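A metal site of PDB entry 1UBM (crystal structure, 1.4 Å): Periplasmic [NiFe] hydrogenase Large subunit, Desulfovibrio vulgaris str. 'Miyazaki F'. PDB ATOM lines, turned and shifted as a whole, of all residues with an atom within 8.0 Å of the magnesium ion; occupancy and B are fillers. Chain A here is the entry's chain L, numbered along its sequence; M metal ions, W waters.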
ATOM      1  N   PHE A  40     -29.692  32.847  13.919  1.00  0.00           N
ATOM      2  CA  PHE A  40     -28.535  32.497  14.747  1.00  0.00           C
ATOM      3  C   PHE A  40     -28.395  33.483  15.912  1.00  0.00           C
ATOM      4  O   PHE A  40     -28.628  34.690  15.716  1.00  0.00           O
ATOM      5  CB  PHE A  40     -27.282  32.467  13.885  1.00  0.00           C
ATOM      6  CG  PHE A  40     -25.984  32.327  14.605  1.00  0.00           C
ATOM      7  CD1 PHE A  40     -25.523  31.092  14.953  1.00  0.00           C
ATOM      8  CD2 PHE A  40     -25.196  33.415  14.942  1.00  0.00           C
ATOM      9  CE1 PHE A  40     -24.333  30.878  15.629  1.00  0.00           C
ATOM     10  CE2 PHE A  40     -23.993  33.219  15.619  1.00  0.00           C
ATOM     11  CZ  PHE A  40     -23.530  31.961  15.932  1.00  0.00           C
ATOM     12  N   GLU A  44     -22.861  30.068  22.205  1.00  0.00           N
ATOM     13  CA  GLU A  44     -21.589  29.377  22.471  1.00  0.00           C
ATOM     14  C   GLU A  44     -20.423  30.371  22.424  1.00  0.00           C
ATOM     15  O   GLU A  44     -19.453  30.266  23.172  1.00  0.00           O
ATOM     16  CB  GLU A  44     -21.350  28.226  21.481  1.00  0.00           C
ATOM     17  CG  GLU A  44     -22.218  26.992  21.693  1.00  0.00           C
ATOM     18  CD  GLU A  44     -22.503  26.204  20.436  1.00  0.00           C
ATOM     19  OE1 GLU A  44     -22.310  26.769  19.334  1.00  0.00           O
ATOM     20  OE2 GLU A  44     -22.947  25.038  20.620  1.00  0.00           O
ATOM     21  N   GLU A 319     -20.199  17.068  14.693  1.00  0.00           N
ATOM     22  CA  GLU A 319     -21.087  18.056  14.119  1.00  0.00           C
ATOM     23  C   GLU A 319     -20.442  18.638  12.847  1.00  0.00           C
ATOM     24  O   GLU A 319     -19.349  19.196  12.864  1.00  0.00           O
ATOM     25  CB  GLU A 319     -21.479  19.205  15.051  1.00  0.00           C
ATOM     26  CG  GLU A 319     -22.156  18.763  16.333  1.00  0.00           C
ATOM     27  CD  GLU A 319     -22.628  19.958  17.125  1.00  0.00           C
ATOM     28  OE1 GLU A 319     -23.827  20.285  17.024  1.00  0.00           O
ATOM     29  OE2 GLU A 319     -21.758  20.549  17.818  1.00  0.00           O
ATOM     30  N   TYR A 326     -21.258  28.164   8.512  1.00  0.00           N
ATOM     31  CA  TYR A 326     -20.093  28.279   9.358  1.00  0.00           C
ATOM     32  C   TYR A 326     -18.888  28.132   8.425  1.00  0.00           C
ATOM     33  O   TYR A 326     -19.013  27.649   7.300  1.00  0.00           O
ATOM     34  CB  TYR A 326     -20.008  27.265  10.524  1.00  0.00           C
ATOM     35  CG  TYR A 326     -21.236  27.425  11.395  1.00  0.00           C
ATOM     36  CD1 TYR A 326     -22.374  26.645  11.196  1.00  0.00           C
ATOM     37  CD2 TYR A 326     -21.217  28.394  12.397  1.00  0.00           C
ATOM     38  CE1 TYR A 326     -23.491  26.810  11.995  1.00  0.00           C
ATOM     39  CE2 TYR A 326     -22.336  28.549  13.175  1.00  0.00           C
ATOM     40  CZ  TYR A 326     -23.457  27.773  12.993  1.00  0.00           C
ATOM     41  OH  TYR A 326     -24.539  27.995  13.817  1.00  0.00           O
ATOM     42  N   PRO A 334     -17.794  17.702  19.880  1.00  0.00           N
ATOM     43  CA  PRO A 334     -18.109  18.921  20.680  1.00  0.00           C
ATOM     44  C   PRO A 334     -17.049  19.398  21.656  1.00  0.00           C
ATOM     45  O   PRO A 334     -16.958  20.566  21.967  1.00  0.00           O
ATOM     46  CB  PRO A 334     -19.384  18.542  21.437  1.00  0.00           C
ATOM     47  CG  PRO A 334     -19.943  17.402  20.717  1.00  0.00           C
ATOM     48  CD  PRO A 334     -18.850  16.704  19.991  1.00  0.00           C
ATOM     49  N   GLY A 337     -15.261  21.561  19.597  1.00  0.00           N
ATOM     50  CA  GLY A 337     -16.172  22.236  18.707  1.00  0.00           C
ATOM     51  C   GLY A 337     -15.773  23.640  18.332  1.00  0.00           C
ATOM     52  O   GLY A 337     -14.945  24.262  19.011  1.00  0.00           O
ATOM     53  N   GLN A 338     -16.413  24.100  17.247  1.00  0.00           N
ATOM     54  CA  GLN A 338     -16.136  25.427  16.697  1.00  0.00           C
ATOM     55  C   GLN A 338     -17.422  26.082  16.247  1.00  0.00           C
ATOM     56  O   GLN A 338     -18.230  25.393  15.626  1.00  0.00           O
ATOM     57  CB  GLN A 338     -15.204  25.387  15.463  1.00  0.00           C
ATOM     58  CG  GLN A 338     -13.811  24.945  15.793  1.00  0.00           C
ATOM     59  CD  GLN A 338     -12.912  24.908  14.545  1.00  0.00           C
ATOM     60  OE1 GLN A 338     -11.872  25.544  14.513  1.00  0.00           O
ATOM     61  NE2 GLN A 338     -13.402  24.168  13.567  1.00  0.00           N
ATOM     62  N   THR A 339     -17.570  27.358  16.553  1.00  0.00           N
ATOM     63  CA  THR A 339     -18.787  28.095  16.159  1.00  0.00           C
ATOM     64  C   THR A 339     -18.360  29.435  15.554  1.00  0.00           C
ATOM     65  O   THR A 339     -18.205  30.457  16.199  1.00  0.00           O
ATOM     66  CB  THR A 339     -19.728  28.286  17.356  1.00  0.00           C
ATOM     67  OG1 THR A 339     -20.009  27.006  17.944  1.00  0.00           O
ATOM     68  CG2 THR A 339     -21.048  28.872  16.920  1.00  0.00           C
ATOM     69  N   TRP A 354     -28.464  27.592   9.675  1.00  0.00           N
ATOM     70  CA  TRP A 354     -27.642  27.979  10.798  1.00  0.00           C
ATOM     71  C   TRP A 354     -27.379  26.882  11.811  1.00  0.00           C
ATOM     72  O   TRP A 354     -26.622  26.927  12.778  1.00  0.00           O
ATOM     73  CB  TRP A 354     -28.234  29.168  11.575  1.00  0.00           C
ATOM     74  CG  TRP A 354     -28.059  30.489  10.900  1.00  0.00           C
ATOM     75  CD1 TRP A 354     -29.030  31.261  10.343  1.00  0.00           C
ATOM     76  CD2 TRP A 354     -26.820  31.178  10.717  1.00  0.00           C
ATOM     77  NE1 TRP A 354     -28.492  32.406   9.819  1.00  0.00           N
ATOM     78  CE2 TRP A 354     -27.122  32.378  10.035  1.00  0.00           C
ATOM     79  CE3 TRP A 354     -25.497  30.920  11.045  1.00  0.00           C
ATOM     80  CZ2 TRP A 354     -26.131  33.307   9.685  1.00  0.00           C
ATOM     81  CZ3 TRP A 354     -24.514  31.833  10.708  1.00  0.00           C
ATOM     82  CH2 TRP A 354     -24.845  33.021  10.030  1.00  0.00           C
ATOM     83  N   MET A 355     -27.993  25.748  11.713  1.00  0.00           N
ATOM     84  CA  MET A 355     -27.817  24.518  12.416  1.00  0.00           C
ATOM     85  C   MET A 355     -26.623  23.781  11.830  1.00  0.00           C
ATOM     86  O   MET A 355     -26.465  23.703  10.620  1.00  0.00           O
ATOM     87  CB  MET A 355     -28.996  23.537  12.360  1.00  0.00           C
ATOM     88  CG  MET A 355     -30.219  23.958  13.134  1.00  0.00           C
ATOM     89  SD  MET A 355     -31.303  22.546  13.486  1.00  0.00           S
ATOM     90  CE  MET A 355     -32.815  23.483  13.882  1.00  0.00           C
ATOM     91  N   LYS A 356     -25.851  23.223  12.749  1.00  0.00           N
ATOM     92  CA  LYS A 356     -24.857  22.221  12.380  1.00  0.00           C
ATOM     93  C   LYS A 356     -25.577  20.881  12.139  1.00  0.00           C
ATOM     94  O   LYS A 356     -26.753  20.802  12.472  1.00  0.00           O
ATOM     95  CB  LYS A 356     -23.799  22.110  13.446  1.00  0.00           C
ATOM     96  CG  LYS A 356     -23.039  23.395  13.781  1.00  0.00           C
ATOM     97  CD  LYS A 356     -22.088  23.254  14.974  1.00  0.00           C
ATOM     98  CE  LYS A 356     -21.346  24.508  15.335  1.00  0.00           C
ATOM     99  NZ  LYS A 356     -20.665  24.333  16.668  1.00  0.00           N
ATOM    100  N   PRO A 358     -25.281  17.218  13.191  1.00  0.00           N
ATOM    101  CA  PRO A 358     -24.664  16.199  14.031  1.00  0.00           C
ATOM    102  C   PRO A 358     -24.838  14.825  13.382  1.00  0.00           C
ATOM    103  O   PRO A 358     -25.896  14.467  12.835  1.00  0.00           O
ATOM    104  CB  PRO A 358     -25.462  16.260  15.341  1.00  0.00           C
ATOM    105  CG  PRO A 358     -26.170  17.574  15.288  1.00  0.00           C
ATOM    106  CD  PRO A 358     -26.504  17.760  13.802  1.00  0.00           C
ATOM    107  N   SER A 465     -27.023  17.395  24.787  1.00  0.00           N
ATOM    108  CA  SER A 465     -25.745  17.338  25.477  1.00  0.00           C
ATOM    109  C   SER A 465     -25.082  18.710  25.484  1.00  0.00           C
ATOM    110  O   SER A 465     -25.096  19.402  24.484  1.00  0.00           O
ATOM    111  CB  SER A 465     -24.821  16.272  24.863  1.00  0.00           C
ATOM    112  OG  SER A 465     -24.713  16.359  23.477  1.00  0.00           O
ATOM    113  N   TRP A 467     -21.341  20.412  26.617  1.00  0.00           N
ATOM    114  CA  TRP A 467     -19.927  20.035  26.646  1.00  0.00           C
ATOM    115  C   TRP A 467     -19.079  21.251  27.004  1.00  0.00           C
ATOM    116  O   TRP A 467     -19.105  22.264  26.343  1.00  0.00           O
ATOM    117  CB  TRP A 467     -19.536  19.514  25.281  1.00  0.00           C
ATOM    118  CG  TRP A 467     -20.332  18.388  24.706  1.00  0.00           C
ATOM    119  CD1 TRP A 467     -21.559  18.509  24.154  1.00  0.00           C
ATOM    120  CD2 TRP A 467     -19.983  16.991  24.635  1.00  0.00           C
ATOM    121  NE1 TRP A 467     -22.017  17.287  23.716  1.00  0.00           N
ATOM    122  CE2 TRP A 467     -21.072  16.338  23.997  1.00  0.00           C
ATOM    123  CE3 TRP A 467     -18.873  16.222  25.030  1.00  0.00           C
ATOM    124  CZ2 TRP A 467     -21.064  14.968  23.756  1.00  0.00           C
ATOM    125  CZ3 TRP A 467     -18.879  14.869  24.784  1.00  0.00           C
ATOM    126  CH2 TRP A 467     -19.962  14.271  24.164  1.00  0.00           C
ATOM    127  N   PHE A 478     -17.472  25.869  25.171  1.00  0.00           N
ATOM    128  CA  PHE A 478     -18.767  25.370  25.610  1.00  0.00           C
ATOM    129  C   PHE A 478     -19.570  25.100  24.334  1.00  0.00           C
ATOM    130  O   PHE A 478     -19.742  26.009  23.519  1.00  0.00           O
ATOM    131  CB  PHE A 478     -19.512  26.340  26.514  1.00  0.00           C
ATOM    132  CG  PHE A 478     -20.549  25.645  27.408  1.00  0.00           C
ATOM    133  CD1 PHE A 478     -21.740  25.219  26.860  1.00  0.00           C
ATOM    134  CD2 PHE A 478     -20.309  25.427  28.740  1.00  0.00           C
ATOM    135  CE1 PHE A 478     -22.705  24.590  27.639  1.00  0.00           C
ATOM    136  CE2 PHE A 478     -21.257  24.808  29.542  1.00  0.00           C
ATOM    137  CZ  PHE A 478     -22.446  24.375  28.987  1.00  0.00           C
ATOM    138  N   GLN A 479     -19.993  23.861  24.196  1.00  0.00           N
ATOM    139  CA  GLN A 479     -20.742  23.478  23.005  1.00  0.00           C
ATOM    140  C   GLN A 479     -22.046  22.792  23.410  1.00  0.00           C
ATOM    141  O   GLN A 479     -22.046  21.899  24.245  1.00  0.00           O
ATOM    142  CB  GLN A 479     -19.928  22.556  22.101  1.00  0.00           C
ATOM    143  CG  GLN A 479     -18.692  23.219  21.527  1.00  0.00           C
ATOM    144  CD  GLN A 479     -18.992  24.234  20.440  1.00  0.00           C
ATOM    145  OE1 GLN A 479     -19.927  24.009  19.670  1.00  0.00           O
ATOM    146  NE2 GLN A 479     -18.189  25.315  20.430  1.00  0.00           N
ATOM    147  N   LEU A 480     -23.119  23.236  22.758  1.00  0.00           N
ATOM    148  CA  LEU A 480     -24.419  22.627  22.902  1.00  0.00           C
ATOM    149  C   LEU A 480     -24.682  21.783  21.662  1.00  0.00           C
ATOM    150  O   LEU A 480     -24.505  22.259  20.587  1.00  0.00           O
ATOM    151  CB  LEU A 480     -25.551  23.630  23.043  1.00  0.00           C
ATOM    152  CG  LEU A 480     -25.613  24.485  24.306  1.00  0.00           C
ATOM    153  CD1 LEU A 480     -24.480  25.462  24.309  1.00  0.00           C
ATOM    154  CD2 LEU A 480     -26.969  25.194  24.369  1.00  0.00           C
ATOM    155  N   VAL A 481     -25.097  20.536  21.806  1.00  0.00           N
ATOM    156  CA  VAL A 481     -25.625  19.687  20.737  1.00  0.00           C
ATOM    157  C   VAL A 481     -27.036  19.263  21.154  1.00  0.00           C
ATOM    158  O   VAL A 481     -27.167  18.538  22.158  1.00  0.00           O
ATOM    159  CB  VAL A 481     -24.733  18.475  20.501  1.00  0.00           C
ATOM    160  CG1 VAL A 481     -25.171  17.805  19.211  1.00  0.00           C
ATOM    161  CG2 VAL A 481     -23.272  18.879  20.476  1.00  0.00           C
ATOM    162  N   VAL A 482     -28.017  19.787  20.393  1.00  0.00           N
ATOM    163  CA  VAL A 482     -29.391  19.810  20.897  1.00  0.00           C
ATOM    164  C   VAL A 482     -30.289  18.877  20.074  1.00  0.00           C
ATOM    165  O   VAL A 482     -29.957  18.660  18.909  1.00  0.00           O
ATOM    166  CB  VAL A 482     -29.854  21.270  20.872  1.00  0.00           C
ATOM    167  CG1 VAL A 482     -31.140  21.545  21.585  1.00  0.00           C
ATOM    168  CG2 VAL A 482     -28.836  22.146  21.601  1.00  0.00           C
ATOM    169  N   THR A 485     -31.121  19.858  16.657  1.00  0.00           N
ATOM    170  CA  THR A 485     -29.933  19.903  15.802  1.00  0.00           C
ATOM    171  C   THR A 485     -29.791  18.566  15.066  1.00  0.00           C
ATOM    172  O   THR A 485     -29.627  18.562  13.842  1.00  0.00           O
ATOM    173  CB  THR A 485     -28.640  20.215  16.607  1.00  0.00           C
ATOM    174  OG1 THR A 485     -28.853  21.191  17.633  1.00  0.00           O
ATOM    175  CG2 THR A 485     -27.588  20.784  15.654  1.00  0.00           C
ATOM    176  N   CYS A 531     -33.452  26.113  19.965  1.00  0.00           N
ATOM    177  CA  CYS A 531     -32.690  24.981  20.458  1.00  0.00           C
ATOM    178  C   CYS A 531     -31.653  24.508  19.465  1.00  0.00           C
ATOM    179  O   CYS A 531     -30.477  24.304  19.754  1.00  0.00           O
ATOM    180  CB  CYS A 531     -33.620  23.784  20.773  1.00  0.00           C
ATOM    181  SG  CYS A 531     -34.150  23.754  22.495  1.00  0.00           S
ATOM    182  N   GLY A 532     -32.114  24.270  18.245  1.00  0.00           N
ATOM    183  CA  GLY A 532     -31.244  23.653  17.259  1.00  0.00           C
ATOM    184  C   GLY A 532     -30.007  24.453  16.923  1.00  0.00           C
ATOM    185  O   GLY A 532     -28.931  23.892  16.673  1.00  0.00           O
ATOM    186  N   VAL A 533     -30.158  25.763  16.851  1.00  0.00           N
ATOM    187  CA  VAL A 533     -29.136  26.685  16.403  1.00  0.00           C
ATOM    188  C   VAL A 533     -28.403  27.337  17.554  1.00  0.00           C
ATOM    189  O   VAL A 533     -27.148  27.419  17.570  1.00  0.00           O
ATOM    190  CB  VAL A 533     -29.667  27.852  15.557  1.00  0.00           C
ATOM    191  CG1 VAL A 533     -28.476  28.757  15.233  1.00  0.00           C
ATOM    192  CG2 VAL A 533     -30.399  27.380  14.316  1.00  0.00           C
ATOM    193  N   HIS A 534     -29.083  27.728  18.632  1.00  0.00           N
ATOM    194  CA  HIS A 534     -28.573  28.403  19.795  1.00  0.00           C
ATOM    195  C   HIS A 534     -27.543  29.484  19.393  1.00  0.00           C
ATOM    196  O   HIS A 534     -27.918  30.350  18.303  1.00  0.00           O
ATOM    197  CB  HIS A 534     -27.980  27.469  20.846  1.00  0.00           C
ATOM    198  CG  HIS A 534     -27.195  26.307  20.357  1.00  0.00           C
ATOM    199  ND1 HIS A 534     -27.899  25.217  19.845  1.00  0.00           N
ATOM    200  CD2 HIS A 534     -25.903  26.037  20.128  1.00  0.00           C
ATOM    201  CE1 HIS A 534     -27.033  24.301  19.411  1.00  0.00           C
ATOM    202  NE2 HIS A 534     -25.819  24.815  19.578  1.00  0.00           N
ATOM    203  OXT HIS A 534     -26.378  29.778  19.806  1.00  0.00           O
HETATM  204 MG    MG M   1     -23.968  23.763  19.166  1.00  0.00          MG
HETATM  205  O   HOH W   1     -24.891  22.550  17.678  1.00  0.00           O
HETATM  206  O   HOH W   2     -23.316  25.073  17.682  1.00  0.00           O
HETATM  207  O   HOH W   3     -22.146  22.914  18.789  1.00  0.00           O
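The magnesium ion is bound by water W3 (2.0 Å), water W2 (2.1 Å), water W1 (2.1 Å), O of Leu 480 (2.1 Å), NE2 of His 534 (2.2 Å) and OE2 of Glu 44 (2.2 Å).
The magnesium ion has six donor atoms within binding distance.
Within 4 Å of the magnesium ion: Glu 44, Leu 480 and His 534.
Water W2 lies within hydrogen-bond range of OE1 of Glu 44 (2.6 Å) and NZ of Lys 356 (2.9 Å).
Water W3 lies within hydrogen-bond range of the side-chain carboxylate of Glu 319 (2.6 Å), the side-chain amide oxygen of Gln 479 (2.6 Å) and the side-chain amino group of Lys 356 (3.0 Å).
ND1 of His 534 lies within hydrogen-bond range of O of Cys 531, 2.7 Å away.
The side-chain carboxylate (OE2) of Glu 44 lies close to the side-chain amide oxygen (OE1) of Gln 479 (3.3 Å).
The side-chain carboxylate of Glu 44 lies within salt-bridge range of the side-chain amino group of Lys 356 (3.97 Å).
OG1 of Thr 339 lies within hydrogen-bond range of OE1 of Glu 44.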
